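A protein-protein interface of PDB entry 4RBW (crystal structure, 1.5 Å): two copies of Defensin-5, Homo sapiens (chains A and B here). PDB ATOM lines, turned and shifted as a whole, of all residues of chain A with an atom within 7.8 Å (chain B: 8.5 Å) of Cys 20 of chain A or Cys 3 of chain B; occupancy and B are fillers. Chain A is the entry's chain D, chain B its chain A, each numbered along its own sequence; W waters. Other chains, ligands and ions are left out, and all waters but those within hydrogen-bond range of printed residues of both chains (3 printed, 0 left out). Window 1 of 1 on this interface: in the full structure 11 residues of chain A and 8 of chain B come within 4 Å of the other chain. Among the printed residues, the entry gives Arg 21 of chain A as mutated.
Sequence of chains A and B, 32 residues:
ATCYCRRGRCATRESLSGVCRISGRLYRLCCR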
ATOM      1  N   CYS A   3       6.594  -5.429 -26.212  1.00  0.00           N
ATOM      2  CA  CYS A   3       5.474  -4.580 -26.573  1.00  0.00           C
ATOM      3  C   CYS A   3       5.904  -3.147 -26.601  1.00  0.00           C
ATOM      4  O   CYS A   3       6.670  -2.680 -25.734  1.00  0.00           O
ATOM      5  CB  CYS A   3       4.364  -4.698 -25.562  1.00  0.00           C
ATOM      6  SG  CYS A   3       3.588  -6.356 -25.492  1.00  0.00           S
ATOM      7  N   TYR A   4       5.268  -2.400 -27.503  1.00  0.00           N
ATOM      8  CA  TYR A   4       5.524  -0.974 -27.686  1.00  0.00           C
ATOM      9  C   TYR A   4       4.231  -0.234 -27.718  1.00  0.00           C
ATOM     10  O   TYR A   4       3.203  -0.746 -28.210  1.00  0.00           O
ATOM     11  CB  TYR A   4       6.352  -0.690 -28.949  1.00  0.00           C
ATOM     12  CG  TYR A   4       7.755  -1.213 -28.926  1.00  0.00           C
ATOM     13  CD1 TYR A   4       8.145  -2.193 -29.804  1.00  0.00           C
ATOM     14  CD2 TYR A   4       8.687  -0.749 -28.027  1.00  0.00           C
ATOM     15  CE1 TYR A   4       9.441  -2.702 -29.796  1.00  0.00           C
ATOM     16  CE2 TYR A   4       9.988  -1.253 -28.013  1.00  0.00           C
ATOM     17  CZ  TYR A   4      10.349  -2.238 -28.902  1.00  0.00           C
ATOM     18  OH  TYR A   4      11.650  -2.751 -28.876  1.00  0.00           O
ATOM     19  N   CYS A   5       4.225   0.988 -27.197  1.00  0.00           N
ATOM     20  CA  CYS A   5       3.075   1.847 -27.374  1.00  0.00           C
ATOM     21  C   CYS A   5       3.292   2.785 -28.545  1.00  0.00           C
ATOM     22  O   CYS A   5       4.227   3.568 -28.547  1.00  0.00           O
ATOM     23  CB  CYS A   5       2.859   2.642 -26.163  1.00  0.00           C
ATOM     24  SG  CYS A   5       2.570   1.625 -24.701  1.00  0.00           S
ATOM     25  N   ARG A   6       2.437   2.669 -29.558  1.00  0.00           N
ATOM     26  CA  ARG A   6       2.641   3.370 -30.806  1.00  0.00           C
ATOM     27  C   ARG A   6       1.563   4.396 -31.128  1.00  0.00           C
ATOM     28  O   ARG A   6       0.389   4.235 -30.857  1.00  0.00           O
ATOM     29  CB  ARG A   6       2.702   2.352 -31.915  1.00  0.00           C
ATOM     30  CG  ARG A   6       3.834   1.370 -31.803  1.00  0.00           C
ATOM     31  CD  ARG A   6       4.226   0.862 -33.188  1.00  0.00           C
ATOM     32  NE  ARG A   6       5.288  -0.113 -33.111  1.00  0.00           N
ATOM     33  CZ  ARG A   6       6.583   0.158 -32.994  1.00  0.00           C
ATOM     34  NH1 ARG A   6       7.036   1.421 -32.952  1.00  0.00           N
ATOM     35  NH2 ARG A   6       7.457  -0.870 -32.898  1.00  0.00           N
ATOM     36  N   LEU A  16      -1.753  -6.028 -32.842  1.00  0.00           N
ATOM     37  CA  LEU A  16      -2.497  -5.106 -31.995  1.00  0.00           C
ATOM     38  C   LEU A  16      -3.026  -5.862 -30.824  1.00  0.00           C
ATOM     39  O   LEU A  16      -3.832  -6.791 -30.979  1.00  0.00           O
ATOM     40  CB  LEU A  16      -3.616  -4.422 -32.774  1.00  0.00           C
ATOM     41  CG  LEU A  16      -4.419  -3.409 -31.945  1.00  0.00           C
ATOM     42  CD1 LEU A  16      -3.581  -2.276 -31.346  1.00  0.00           C
ATOM     43  CD2 LEU A  16      -5.635  -2.869 -32.719  1.00  0.00           C
ATOM     44  N   SER A  17      -2.599  -5.477 -29.643  1.00  0.00           N
ATOM     45  CA  SER A  17      -2.913  -6.280 -28.435  1.00  0.00           C
ATOM     46  C   SER A  17      -3.720  -5.479 -27.404  1.00  0.00           C
ATOM     47  O   SER A  17      -4.061  -6.001 -26.300  1.00  0.00           O
ATOM     48  CB  SER A  17      -1.623  -6.779 -27.812  1.00  0.00           C
ATOM     49  OG  SER A  17      -0.850  -7.536 -28.755  1.00  0.00           O
ATOM     50  N   GLY A  18      -4.030  -4.243 -27.727  1.00  0.00           N
ATOM     51  CA  GLY A  18      -4.824  -3.408 -26.842  1.00  0.00           C
ATOM     52  C   GLY A  18      -4.431  -1.959 -26.982  1.00  0.00           C
ATOM     53  O   GLY A  18      -4.044  -1.529 -28.062  1.00  0.00           O
ATOM     54  N   VAL A  19      -4.529  -1.215 -25.895  1.00  0.00           N
ATOM     55  CA  VAL A  19      -4.182   0.196 -25.863  1.00  0.00           C
ATOM     56  C   VAL A  19      -3.239   0.481 -24.711  1.00  0.00           C
ATOM     57  O   VAL A  19      -3.198  -0.258 -23.741  1.00  0.00           O
ATOM     58  CB  VAL A  19      -5.374   1.142 -25.816  1.00  0.00           C
ATOM     59  CG1 VAL A  19      -6.224   0.963 -27.041  1.00  0.00           C
ATOM     60  CG2 VAL A  19      -6.180   0.959 -24.534  1.00  0.00           C
ATOM     61  N   CYS A  20      -2.509   1.600 -24.859  1.00  0.00           N
ATOM     62  CA  CYS A  20      -1.744   2.161 -23.739  1.00  0.00           C
ATOM     63  C   CYS A  20      -2.348   3.511 -23.388  1.00  0.00           C
ATOM     64  O   CYS A  20      -2.582   4.326 -24.270  1.00  0.00           O
ATOM     65  CB  CYS A  20      -0.269   2.436 -24.059  1.00  0.00           C
ATOM     66  SG  CYS A  20       0.571   1.046 -24.846  1.00  0.00           S
ATOM     67  N   ARG A  21      -2.463   3.799 -22.096  1.00  0.00           N
ATOM     68  CA  ARG A  21      -3.122   4.984 -21.592  1.00  0.00           C
ATOM     69  C   ARG A  21      -2.242   5.737 -20.613  1.00  0.00           C
ATOM     70  O   ARG A  21      -1.579   5.146 -19.802  1.00  0.00           O
ATOM     71  CB  ARG A  21      -4.407   4.543 -20.884  1.00  0.00           C
ATOM     72  CG  ARG A  21      -5.251   5.618 -20.250  1.00  0.00           C
ATOM     73  CD  ARG A  21      -5.750   6.537 -21.308  1.00  0.00           C
ATOM     74  NE  ARG A  21      -6.862   7.278 -20.820  1.00  0.00           N
ATOM     75  CZ  ARG A  21      -7.253   8.475 -21.259  1.00  0.00           C
ATOM     76  NH1 ARG A  21      -6.578   9.157 -22.177  1.00  0.00           N
ATOM     77  NH2 ARG A  21      -8.378   9.001 -20.743  1.00  0.00           N
ATOM     78  N   ILE A  22      -2.165   7.050 -20.789  1.00  0.00           N
ATOM     79  CA  ILE A  22      -1.734   7.945 -19.716  1.00  0.00           C
ATOM     80  C   ILE A  22      -2.700   9.080 -19.723  1.00  0.00           C
ATOM     81  O   ILE A  22      -3.436   9.273 -20.685  1.00  0.00           O
ATOM     82  CB  ILE A  22      -0.443   8.695 -20.015  1.00  0.00           C
ATOM     83  CG1 ILE A  22       0.335   8.068 -21.152  1.00  0.00           C
ATOM     84  CG2 ILE A  22       0.355   8.947 -18.731  1.00  0.00           C
ATOM     85  CD1 ILE A  22       0.873   9.171 -22.033  1.00  0.00           C
ATOM     86  N   ARG A  25      -3.526  11.008 -23.265  1.00  0.00           N
ATOM     87  CA  ARG A  25      -3.033  10.334 -24.448  1.00  0.00           C
ATOM     88  C   ARG A  25      -3.592   8.880 -24.498  1.00  0.00           C
ATOM     89  O   ARG A  25      -3.835   8.241 -23.493  1.00  0.00           O
ATOM     90  CB  ARG A  25      -1.484  10.371 -24.444  1.00  0.00           C
ATOM     91  CG  ARG A  25      -0.919  11.797 -24.333  1.00  0.00           C
ATOM     92  CD  ARG A  25       0.548  11.989 -24.721  1.00  0.00           C
ATOM     93  NE  ARG A  25       0.857  11.595 -26.111  1.00  0.00           N
ATOM     94  CZ  ARG A  25       1.892  12.045 -26.834  1.00  0.00           C
ATOM     95  NH1 ARG A  25       2.743  12.941 -26.328  1.00  0.00           N
ATOM     96  NH2 ARG A  25       2.081  11.587 -28.083  1.00  0.00           N
ATOM     97  N   LEU A  26      -3.723   8.377 -25.702  1.00  0.00           N
ATOM     98  CA  LEU A  26      -3.989   6.967 -25.942  1.00  0.00           C
ATOM     99  C   LEU A  26      -3.052   6.531 -27.085  1.00  0.00           C
ATOM    100  O   LEU A  26      -2.852   7.280 -28.063  1.00  0.00           O
ATOM    101  CB  LEU A  26      -5.444   6.781 -26.340  1.00  0.00           C
ATOM    102  CG  LEU A  26      -5.838   5.350 -26.427  1.00  0.00           C
ATOM    103  CD1 LEU A  26      -6.124   4.818 -25.040  1.00  0.00           C
ATOM    104  CD2 LEU A  26      -7.054   5.288 -27.301  1.00  0.00           C
ATOM    105  N   TYR A  27      -2.574   5.291 -27.006  1.00  0.00           N
ATOM    106  CA  TYR A  27      -1.702   4.693 -28.050  1.00  0.00           C
ATOM    107  C   TYR A  27      -2.134   3.308 -28.293  1.00  0.00           C
ATOM    108  O   TYR A  27      -2.794   2.682 -27.437  1.00  0.00           O
ATOM    109  CB  TYR A  27      -0.263   4.604 -27.497  1.00  0.00           C
ATOM    110  CG  TYR A  27       0.370   5.896 -27.077  1.00  0.00           C
ATOM    111  CD1 TYR A  27       0.271   6.349 -25.756  1.00  0.00           C
ATOM    112  CD2 TYR A  27       1.201   6.587 -27.942  1.00  0.00           C
ATOM    113  CE1 TYR A  27       0.871   7.494 -25.388  1.00  0.00           C
ATOM    114  CE2 TYR A  27       1.844   7.733 -27.541  1.00  0.00           C
ATOM    115  CZ  TYR A  27       1.691   8.149 -26.272  1.00  0.00           C
ATOM    116  OH  TYR A  27       2.348   9.311 -25.907  1.00  0.00           O
ATOM    117  N   ARG A  28      -1.790   2.770 -29.458  1.00  0.00           N
ATOM    118  CA  ARG A  28      -1.919   1.297 -29.663  1.00  0.00           C
ATOM    119  C   ARG A  28      -0.877   0.554 -28.908  1.00  0.00           C
ATOM    120  O   ARG A  28       0.286   0.960 -28.824  1.00  0.00           O
ATOM    121  CB  ARG A  28      -1.763   0.958 -31.124  1.00  0.00           C
ATOM    122  CG  ARG A  28      -2.895   1.315 -32.041  1.00  0.00           C
ATOM    123  CD  ARG A  28      -2.617   0.848 -33.458  1.00  0.00           C
ATOM    124  NE  ARG A  28      -3.730   0.978 -34.424  1.00  0.00           N
ATOM    125  CZ  ARG A  28      -3.979   2.041 -35.182  1.00  0.00           C
ATOM    126  NH1 ARG A  28      -3.176   3.095 -35.185  1.00  0.00           N
ATOM    127  NH2 ARG A  28      -5.048   1.997 -36.012  1.00  0.00           N
ATOM    128  N   LEU A  29      -1.255  -0.580 -28.361  1.00  0.00           N
ATOM    129  CA  LEU A  29      -0.308  -1.502 -27.756  1.00  0.00           C
ATOM    130  C   LEU A  29       0.018  -2.528 -28.790  1.00  0.00           C
ATOM    131  O   LEU A  29      -0.896  -3.205 -29.227  1.00  0.00           O
ATOM    132  CB  LEU A  29      -0.963  -2.184 -26.577  1.00  0.00           C
ATOM    133  CG  LEU A  29      -0.170  -3.295 -25.874  1.00  0.00           C
ATOM    134  CD1 LEU A  29       1.016  -2.721 -25.206  1.00  0.00           C
ATOM    135  CD2 LEU A  29      -1.012  -4.156 -24.925  1.00  0.00           C
ATOM    136  N   CYS A  30       1.293  -2.678 -29.153  1.00  0.00           N
ATOM    137  CA  CYS A  30       1.731  -3.475 -30.310  1.00  0.00           C
ATOM    138  C   CYS A  30       2.769  -4.458 -29.826  1.00  0.00           C
ATOM    139  O   CYS A  30       3.798  -4.029 -29.291  1.00  0.00           O
ATOM    140  CB  CYS A  30       2.336  -2.551 -31.344  1.00  0.00           C
ATOM    141  SG  CYS A  30       1.215  -1.378 -32.018  1.00  0.00           S
ATOM    142  N   CYS A  31       2.538  -5.768 -30.020  1.00  0.00           N
ATOM    143  CA  CYS A  31       3.367  -6.795 -29.373  1.00  0.00           C
ATOM    144  C   CYS A  31       3.827  -7.836 -30.364  1.00  0.00           C
ATOM    145  O   CYS A  31       3.124  -8.154 -31.311  1.00  0.00           O
ATOM    146  CB  CYS A  31       2.590  -7.487 -28.265  1.00  0.00           C
ATOM    147  SG  CYS A  31       2.051  -6.398 -26.901  1.00  0.00           S
ATOM    148  N   ALA B   1      -5.539  -6.428 -24.072  1.00  0.00           N
ATOM    149  CA  ALA B   1      -4.997  -5.771 -22.862  1.00  0.00           C
ATOM    150  C   ALA B   1      -5.189  -4.245 -22.856  1.00  0.00           C
ATOM    151  O   ALA B   1      -5.381  -3.577 -23.886  1.00  0.00           O
ATOM    152  CB  ALA B   1      -3.523  -6.144 -22.665  1.00  0.00           C
ATOM    153  N   THR B   2      -5.204  -3.694 -21.653  1.00  0.00           N
ATOM    154  CA  THR B   2      -5.107  -2.298 -21.458  1.00  0.00           C
ATOM    155  C   THR B   2      -3.908  -2.103 -20.568  1.00  0.00           C
ATOM    156  O   THR B   2      -3.811  -2.762 -19.489  1.00  0.00           O
ATOM    157  CB  THR B   2      -6.329  -1.733 -20.772  1.00  0.00           C
ATOM    158  OG1 THR B   2      -7.493  -1.942 -21.583  1.00  0.00           O
ATOM    159  CG2 THR B   2      -6.160  -0.216 -20.547  1.00  0.00           C
ATOM    160  N   CYS B   3      -2.981  -1.305 -21.043  1.00  0.00           N
ATOM    161  CA  CYS B   3      -1.829  -0.948 -20.243  1.00  0.00           C
ATOM    162  C   CYS B   3      -1.777   0.516 -19.929  1.00  0.00           C
ATOM    163  O   CYS B   3      -2.318   1.370 -20.640  1.00  0.00           O
ATOM    164  CB  CYS B   3      -0.540  -1.359 -20.895  1.00  0.00           C
ATOM    165  SG  CYS B   3      -0.599  -3.056 -21.568  1.00  0.00           S
ATOM    166  N   TYR B   4      -1.136   0.832 -18.832  1.00  0.00           N
ATOM    167  CA  TYR B   4      -0.939   2.172 -18.374  1.00  0.00           C
ATOM    168  C   TYR B   4       0.545   2.481 -18.350  1.00  0.00           C
ATOM    169  O   TYR B   4       1.324   1.668 -17.899  1.00  0.00           O
ATOM    170  CB  TYR B   4      -1.545   2.287 -16.970  1.00  0.00           C
ATOM    171  CG  TYR B   4      -3.021   2.168 -17.040  1.00  0.00           C
ATOM    172  CD1 TYR B   4      -3.665   0.955 -16.951  1.00  0.00           C
ATOM    173  CD2 TYR B   4      -3.767   3.284 -17.321  1.00  0.00           C
ATOM    174  CE1 TYR B   4      -5.048   0.854 -17.131  1.00  0.00           C
ATOM    175  CE2 TYR B   4      -5.135   3.216 -17.461  1.00  0.00           C
ATOM    176  CZ  TYR B   4      -5.777   2.009 -17.392  1.00  0.00           C
ATOM    177  OH  TYR B   4      -7.156   1.892 -17.562  1.00  0.00           O
ATOM    178  N   CYS B   5       0.906   3.645 -18.825  1.00  0.00           N
ATOM    179  CA  CYS B   5       2.272   4.107 -18.805  1.00  0.00           C
ATOM    180  C   CYS B   5       2.439   4.864 -17.506  1.00  0.00           C
ATOM    181  O   CYS B   5       1.827   5.912 -17.322  1.00  0.00           O
ATOM    182  CB  CYS B   5       2.597   5.008 -20.001  1.00  0.00           C
ATOM    183  SG  CYS B   5       2.514   4.105 -21.592  1.00  0.00           S
ATOM    184  N   ARG B   6       3.279   4.346 -16.612  1.00  0.00           N
ATOM    185  CA  ARG B   6       3.358   4.851 -15.235  1.00  0.00           C
ATOM    186  C   ARG B   6       4.780   5.259 -14.875  1.00  0.00           C
ATOM    187  O   ARG B   6       5.738   4.585 -15.276  1.00  0.00           O
ATOM    188  CB  ARG B   6       2.945   3.723 -14.332  1.00  0.00           C
ATOM    189  CG  ARG B   6       1.521   3.220 -14.522  1.00  0.00           C
ATOM    190  CD  ARG B   6       0.989   2.548 -13.260  1.00  0.00           C
ATOM    191  NE  ARG B   6      -0.372   2.012 -13.388  1.00  0.00           N
ATOM    192  CZ  ARG B   6      -1.509   2.697 -13.467  1.00  0.00           C
ATOM    193  NH1 ARG B   6      -1.552   4.012 -13.397  1.00  0.00           N
ATOM    194  NH2 ARG B   6      -2.645   2.036 -13.580  1.00  0.00           N
ATOM    195  N   CYS B  10       3.860  -0.451 -10.967  1.00  0.00           N
ATOM    196  CA  CYS B  10       2.590  -0.947 -11.395  1.00  0.00           C
ATOM    197  C   CYS B  10       1.610  -1.240 -10.269  1.00  0.00           C
ATOM    198  O   CYS B  10       1.989  -1.498  -9.132  1.00  0.00           O
ATOM    199  CB  CYS B  10       2.763  -2.182 -12.234  1.00  0.00           C
ATOM    200  SG  CYS B  10       3.840  -1.974 -13.677  1.00  0.00           S
ATOM    201  N   GLU B  14      -1.566  -5.332 -11.919  1.00  0.00           N
ATOM    202  CA  GLU B  14      -0.818  -5.134 -13.183  1.00  0.00           C
ATOM    203  C   GLU B  14       0.486  -5.865 -13.198  1.00  0.00           C
ATOM    204  O   GLU B  14       1.052  -6.161 -12.144  1.00  0.00           O
ATOM    205  CB  GLU B  14      -0.554  -3.641 -13.418  1.00  0.00           C
ATOM    206  CG  GLU B  14      -1.793  -2.890 -13.802  1.00  0.00           C
ATOM    207  CD  GLU B  14      -1.705  -1.373 -13.725  1.00  0.00           C
ATOM    208  OE1 GLU B  14      -0.669  -0.786 -13.330  1.00  0.00           O
ATOM    209  OE2 GLU B  14      -2.683  -0.681 -14.076  1.00  0.00           O
ATOM    210  N   SER B  15       0.999  -6.133 -14.378  1.00  0.00           N
ATOM    211  CA  SER B  15       2.343  -6.703 -14.538  1.00  0.00           C
ATOM    212  C   SER B  15       3.201  -5.752 -15.347  1.00  0.00           C
ATOM    213  O   SER B  15       2.726  -5.145 -16.271  1.00  0.00           O
ATOM    214  CB  SER B  15       2.273  -8.059 -15.263  1.00  0.00           C
ATOM    215  OG  SER B  15       1.304  -8.914 -14.665  1.00  0.00           O
ATOM    216  N   LEU B  16       4.476  -5.629 -14.998  1.00  0.00           N
ATOM    217  CA  LEU B  16       5.417  -4.819 -15.777  1.00  0.00           C
ATOM    218  C   LEU B  16       5.669  -5.555 -17.050  1.00  0.00           C
ATOM    219  O   LEU B  16       6.184  -6.686 -17.043  1.00  0.00           O
ATOM    220  CB  LEU B  16       6.700  -4.619 -14.962  1.00  0.00           C
ATOM    221  CG  LEU B  16       7.798  -3.781 -15.601  1.00  0.00           C
ATOM    222  CD1 LEU B  16       7.310  -2.388 -15.927  1.00  0.00           C
ATOM    223  CD2 LEU B  16       9.048  -3.763 -14.692  1.00  0.00           C
ATOM    224  N   SER B  17       5.311  -4.943 -18.170  1.00  0.00           N
ATOM    225  CA  SER B  17       5.332  -5.612 -19.459  1.00  0.00           C
ATOM    226  C   SER B  17       6.260  -4.956 -20.463  1.00  0.00           C
ATOM    227  O   SER B  17       6.300  -5.374 -21.634  1.00  0.00           O
ATOM    228  CB  SER B  17       3.905  -5.710 -20.042  1.00  0.00           C
ATOM    229  OG  SER B  17       3.028  -6.341 -19.140  1.00  0.00           O
ATOM    230  N   GLY B  18       7.009  -3.944 -20.049  1.00  0.00           N
ATOM    231  CA  GLY B  18       7.860  -3.202 -20.993  1.00  0.00           C
ATOM    232  C   GLY B  18       8.007  -1.778 -20.542  1.00  0.00           C
ATOM    233  O   GLY B  18       7.763  -1.475 -19.354  1.00  0.00           O
ATOM    234  N   VAL B  19       8.414  -0.897 -21.475  1.00  0.00           N
ATOM    235  CA  VAL B  19       8.492   0.559 -21.270  1.00  0.00           C
ATOM    236  C   VAL B  19       7.772   1.305 -22.399  1.00  0.00           C
ATOM    237  O   VAL B  19       7.483   0.719 -23.474  1.00  0.00           O
ATOM    238  CB  VAL B  19       9.963   1.022 -21.099  1.00  0.00           C
ATOM    239  CG1 VAL B  19      10.111   2.468 -20.818  1.00  0.00           C
ATOM    240  CG2 VAL B  19      10.610   0.272 -19.945  1.00  0.00           C
ATOM    241  N   CYS B  20       7.344   2.508 -22.078  1.00  0.00           N
ATOM    242  CA  CYS B  20       6.816   3.517 -23.053  1.00  0.00           C
ATOM    243  C   CYS B  20       7.781   4.660 -23.075  1.00  0.00           C
ATOM    244  O   CYS B  20       8.373   5.010 -22.066  1.00  0.00           O
ATOM    245  CB  CYS B  20       5.458   4.160 -22.634  1.00  0.00           C
ATOM    246  SG  CYS B  20       4.364   3.109 -21.704  1.00  0.00           S
ATOM    247  N   ILE B  22       7.522   8.726 -23.891  1.00  0.00           N
ATOM    248  CA  ILE B  22       6.558   9.794 -24.134  1.00  0.00           C
ATOM    249  C   ILE B  22       7.269  11.103 -23.895  1.00  0.00           C
ATOM    250  O   ILE B  22       7.857  11.309 -22.844  1.00  0.00           O
ATOM    251  CB  ILE B  22       5.339   9.670 -23.222  1.00  0.00           C
ATOM    252  CG1 ILE B  22       4.738   8.309 -23.454  1.00  0.00           C
ATOM    253  CG2 ILE B  22       4.330  10.774 -23.536  1.00  0.00           C
ATOM    254  CD1 ILE B  22       3.752   7.860 -22.428  1.00  0.00           C
ATOM    255  N   ARG B  28       7.066   3.052 -17.232  1.00  0.00           N
ATOM    256  CA  ARG B  28       6.741   1.664 -17.107  1.00  0.00           C
ATOM    257  C   ARG B  28       5.483   1.353 -17.886  1.00  0.00           C
ATOM    258  O   ARG B  28       4.541   2.081 -17.797  1.00  0.00           O
ATOM    259  CB  ARG B  28       6.481   1.304 -15.624  1.00  0.00           C
ATOM    260  CG  ARG B  28       7.594   1.536 -14.605  1.00  0.00           C
ATOM    261  CD  ARG B  28       7.085   0.901 -13.317  1.00  0.00           C
ATOM    262  NE  ARG B  28       8.008   0.708 -12.173  1.00  0.00           N
ATOM    263  CZ  ARG B  28       8.413   1.642 -11.295  1.00  0.00           C
ATOM    264  NH1 ARG B  28       8.102   2.916 -11.399  1.00  0.00           N
ATOM    265  NH2 ARG B  28       9.188   1.273 -10.300  1.00  0.00           N
ATOM    266  N   LEU B  29       5.480   0.231 -18.548  1.00  0.00           N
ATOM    267  CA  LEU B  29       4.289  -0.249 -19.225  1.00  0.00           C
ATOM    268  C   LEU B  29       3.677  -1.316 -18.348  1.00  0.00           C
ATOM    269  O   LEU B  29       4.212  -2.398 -18.173  1.00  0.00           O
ATOM    270  CB  LEU B  29       4.642  -0.851 -20.582  1.00  0.00           C
ATOM    271  CG  LEU B  29       3.522  -1.205 -21.550  1.00  0.00           C
ATOM    272  CD1 LEU B  29       2.554  -0.059 -21.824  1.00  0.00           C
ATOM    273  CD2 LEU B  29       4.186  -1.654 -22.842  1.00  0.00           C
ATOM    274  N   CYS B  30       2.550  -0.974 -17.750  1.00  0.00           N
ATOM    275  CA  CYS B  30       1.887  -1.790 -16.749  1.00  0.00           C
ATOM    276  C   CYS B  30       0.575  -2.340 -17.239  1.00  0.00           C
ATOM    277  O   CYS B  30      -0.322  -1.624 -17.505  1.00  0.00           O
ATOM    278  CB  CYS B  30       1.649  -0.952 -15.495  1.00  0.00           C
ATOM    279  SG  CYS B  30       3.125  -0.276 -14.673  1.00  0.00           S
ATOM    280  N   CYS B  31       0.490  -3.645 -17.329  1.00  0.00           N
ATOM    281  CA  CYS B  31      -0.608  -4.251 -18.061  1.00  0.00           C
ATOM    282  C   CYS B  31      -1.442  -5.144 -17.236  1.00  0.00           C
ATOM    283  O   CYS B  31      -0.960  -5.858 -16.383  1.00  0.00           O
ATOM    284  CB  CYS B  31      -0.071  -5.066 -19.219  1.00  0.00           C
ATOM    285  SG  CYS B  31       0.818  -4.086 -20.483  1.00  0.00           S
ATOM    286  N   ARG B  32      -2.713  -5.155 -17.586  1.00  0.00           N
ATOM    287  CA  ARG B  32      -3.585  -6.238 -17.185  1.00  0.00           C
ATOM    288  C   ARG B  32      -4.473  -6.617 -18.368  1.00  0.00           C
ATOM    289  O   ARG B  32      -5.307  -7.530 -18.274  1.00  0.00           O
ATOM    290  CB  ARG B  32      -4.409  -5.823 -15.980  1.00  0.00           C
ATOM    291  CG  ARG B  32      -5.159  -4.519 -16.167  1.00  0.00           C
ATOM    292  CD  ARG B  32      -5.969  -4.181 -14.919  1.00  0.00           C
ATOM    293  NE  ARG B  32      -6.672  -5.334 -14.346  1.00  0.00           N
ATOM    294  CZ  ARG B  32      -7.990  -5.436 -14.162  1.00  0.00           C
ATOM    295  NH1 ARG B  32      -8.819  -4.450 -14.487  1.00  0.00           N
ATOM    296  NH2 ARG B  32      -8.480  -6.552 -13.629  1.00  0.00           N
HETATM  297  O   HOH W   1       6.786   1.738 -26.015  1.00  0.00           O
HETATM  298  O   HOH W   2       8.860  -2.508 -23.898  1.00  0.00           O
HETATM  299  O   HOH W   3       8.219  -5.182 -23.671  1.00  0.00           O
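The backbone NH (N) of Ala 1 of chain B sits at hydrogen-bond distance from the backbone carbonyl oxygen (O) of Ser 17 of chain A (2.7 Å). The backbone carbonyl oxygen of Ala 1 of chain B sits at hydrogen-bond distance from the backbone NH of Val 19 of chain A, 3.2 Å away. The backbone NH (N) of Cys 3 of chain B is in hydrogen-bond range of the backbone carbonyl oxygen (O) of Val 19 of chain A (2.9 Å). The backbone carbonyl oxygen of Cys 3 of chain B is in hydrogen-bond range of the backbone NH of Arg 21 of chain A, 2.8 Å away. The backbone NH (N) of Cys 5 of chain B is in hydrogen-bond range of the backbone carbonyl oxygen (O) of Arg 21 of chain A, 3.1 Å away. SG of Cys 5 of chain A lies close to SG of Cys 20 of chain B (3.8 Å).
SG of Cys 20 of chain A forms a disulfide with SG of Cys 5 of chain A (2.1 Å). The backbone carbonyl oxygen (O) of Tyr 27 of chain A lies within hydrogen-bond range of the backbone NH (N) of Cys 20 of chain A, at 2.8 Å. NH1 of Arg 21 of chain A lies within hydrogen-bond range of O of Arg 25 of chain A, at 3.2 Å. The guanidinium group of Arg 25 of chain A is in hydrogen-bond range of the side-chain hydroxyl of Tyr 27 of chain A, at 2.7 Å.
O of Cys 3 of chain A touches CD2 of Leu 29 of chain B, 3.9 Å away. Cys 5 of chain A touches Cys 5 of chain B (SG to SG, 3.98 Å). SG of Cys 5 of chain A touches CD1 of Leu 29 of chain B, at 3.3 Å. Ala 1 of chain B touches Gly 18 of chain A. Leu 29 of chain B touches Cys 20 of chain A. CA of Tyr 4 of chain B touches O of Arg 21 of chain A, at 3.4 Å. Ile 22 of chain B touches Arg 25 of chain A (CG2 to NH1, 3.9 Å). Ile 22 of chain B touches Tyr 27 of chain A (CG2 to OH, 3.4 Å). Leu 29 of chain A touches Ala 1 of chain B.
Printed residues of chain B within 4 Å of Cys 5 of chain A: Cys 5, Cys 20 and Leu 29. Of chain B, only Ala 1, Thr 2 and Cys 3 come within 4 Å of Val 19 of chain A. Printed residues of chain B within 4 Å of Tyr 27 of chain A: Ile 22 (3.4 Å). Printed residues of chain A within 4 Å of Thr 2 of chain B: Val 19 (3.6 Å). The nearest printed residue of chain A that does not touch Cys 3 of chain B is Ile 22 of chain A (5.7 Å).
Of the 20 printed residues of chain B, 8 touch a printed residue of chain A. Hydrophobic or aromatic side chains of chain B within 4 Å of the printed part of chain A: Ala 1, Tyr 4, Ile 22 and Leu 29. Hydrophobic or aromatic side chains of chain A that line the printed part of chain B: Ile 22, Tyr 27 and Leu 29. Along chain A the printed residues that touch a printed residue of chain B span positions 3 to 29. Among the printed residues, no Asp or Glu carboxylate lies within 4 Å of a Lys or Arg side-chain nitrogen of the other chain.
Cys 3 of chain A touches Leu 29 of chain B, and with the chains exchanged Leu 29 of chain A touches Cys 3 of chain B. Cys 5 of chain A touches Cys 20 of chain B, but with the chains exchanged Cys 20 of chain A does not touch Cys 5 of chain B (4.1 Å). Val 19 of chain A touches Cys 3 of chain B, but with the chains exchanged Cys 3 of chain A does not touch Val 19 of chain B (4.2 Å). 14 positions are printed for both chains. Of the 20 pairs that touch across the chains among the printed residues, 4 have their exchanged pair printed and touching as well.
Water W3 lies within hydrogen-bond range of O of Ser 17 of chain B (2.8 Å) and N of Cys 3 of chain A (3.0 Å). Water W1 lies within hydrogen-bond range of the backbone carbonyl oxygen (O) of Val 19 of chain B (2.8 Å) and the backbone NH (N) of Cys 5 of chain A (2.9 Å). Water W2 lies within hydrogen-bond range of O of Cys 3 of chain A and N of Val 19 of chain B.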
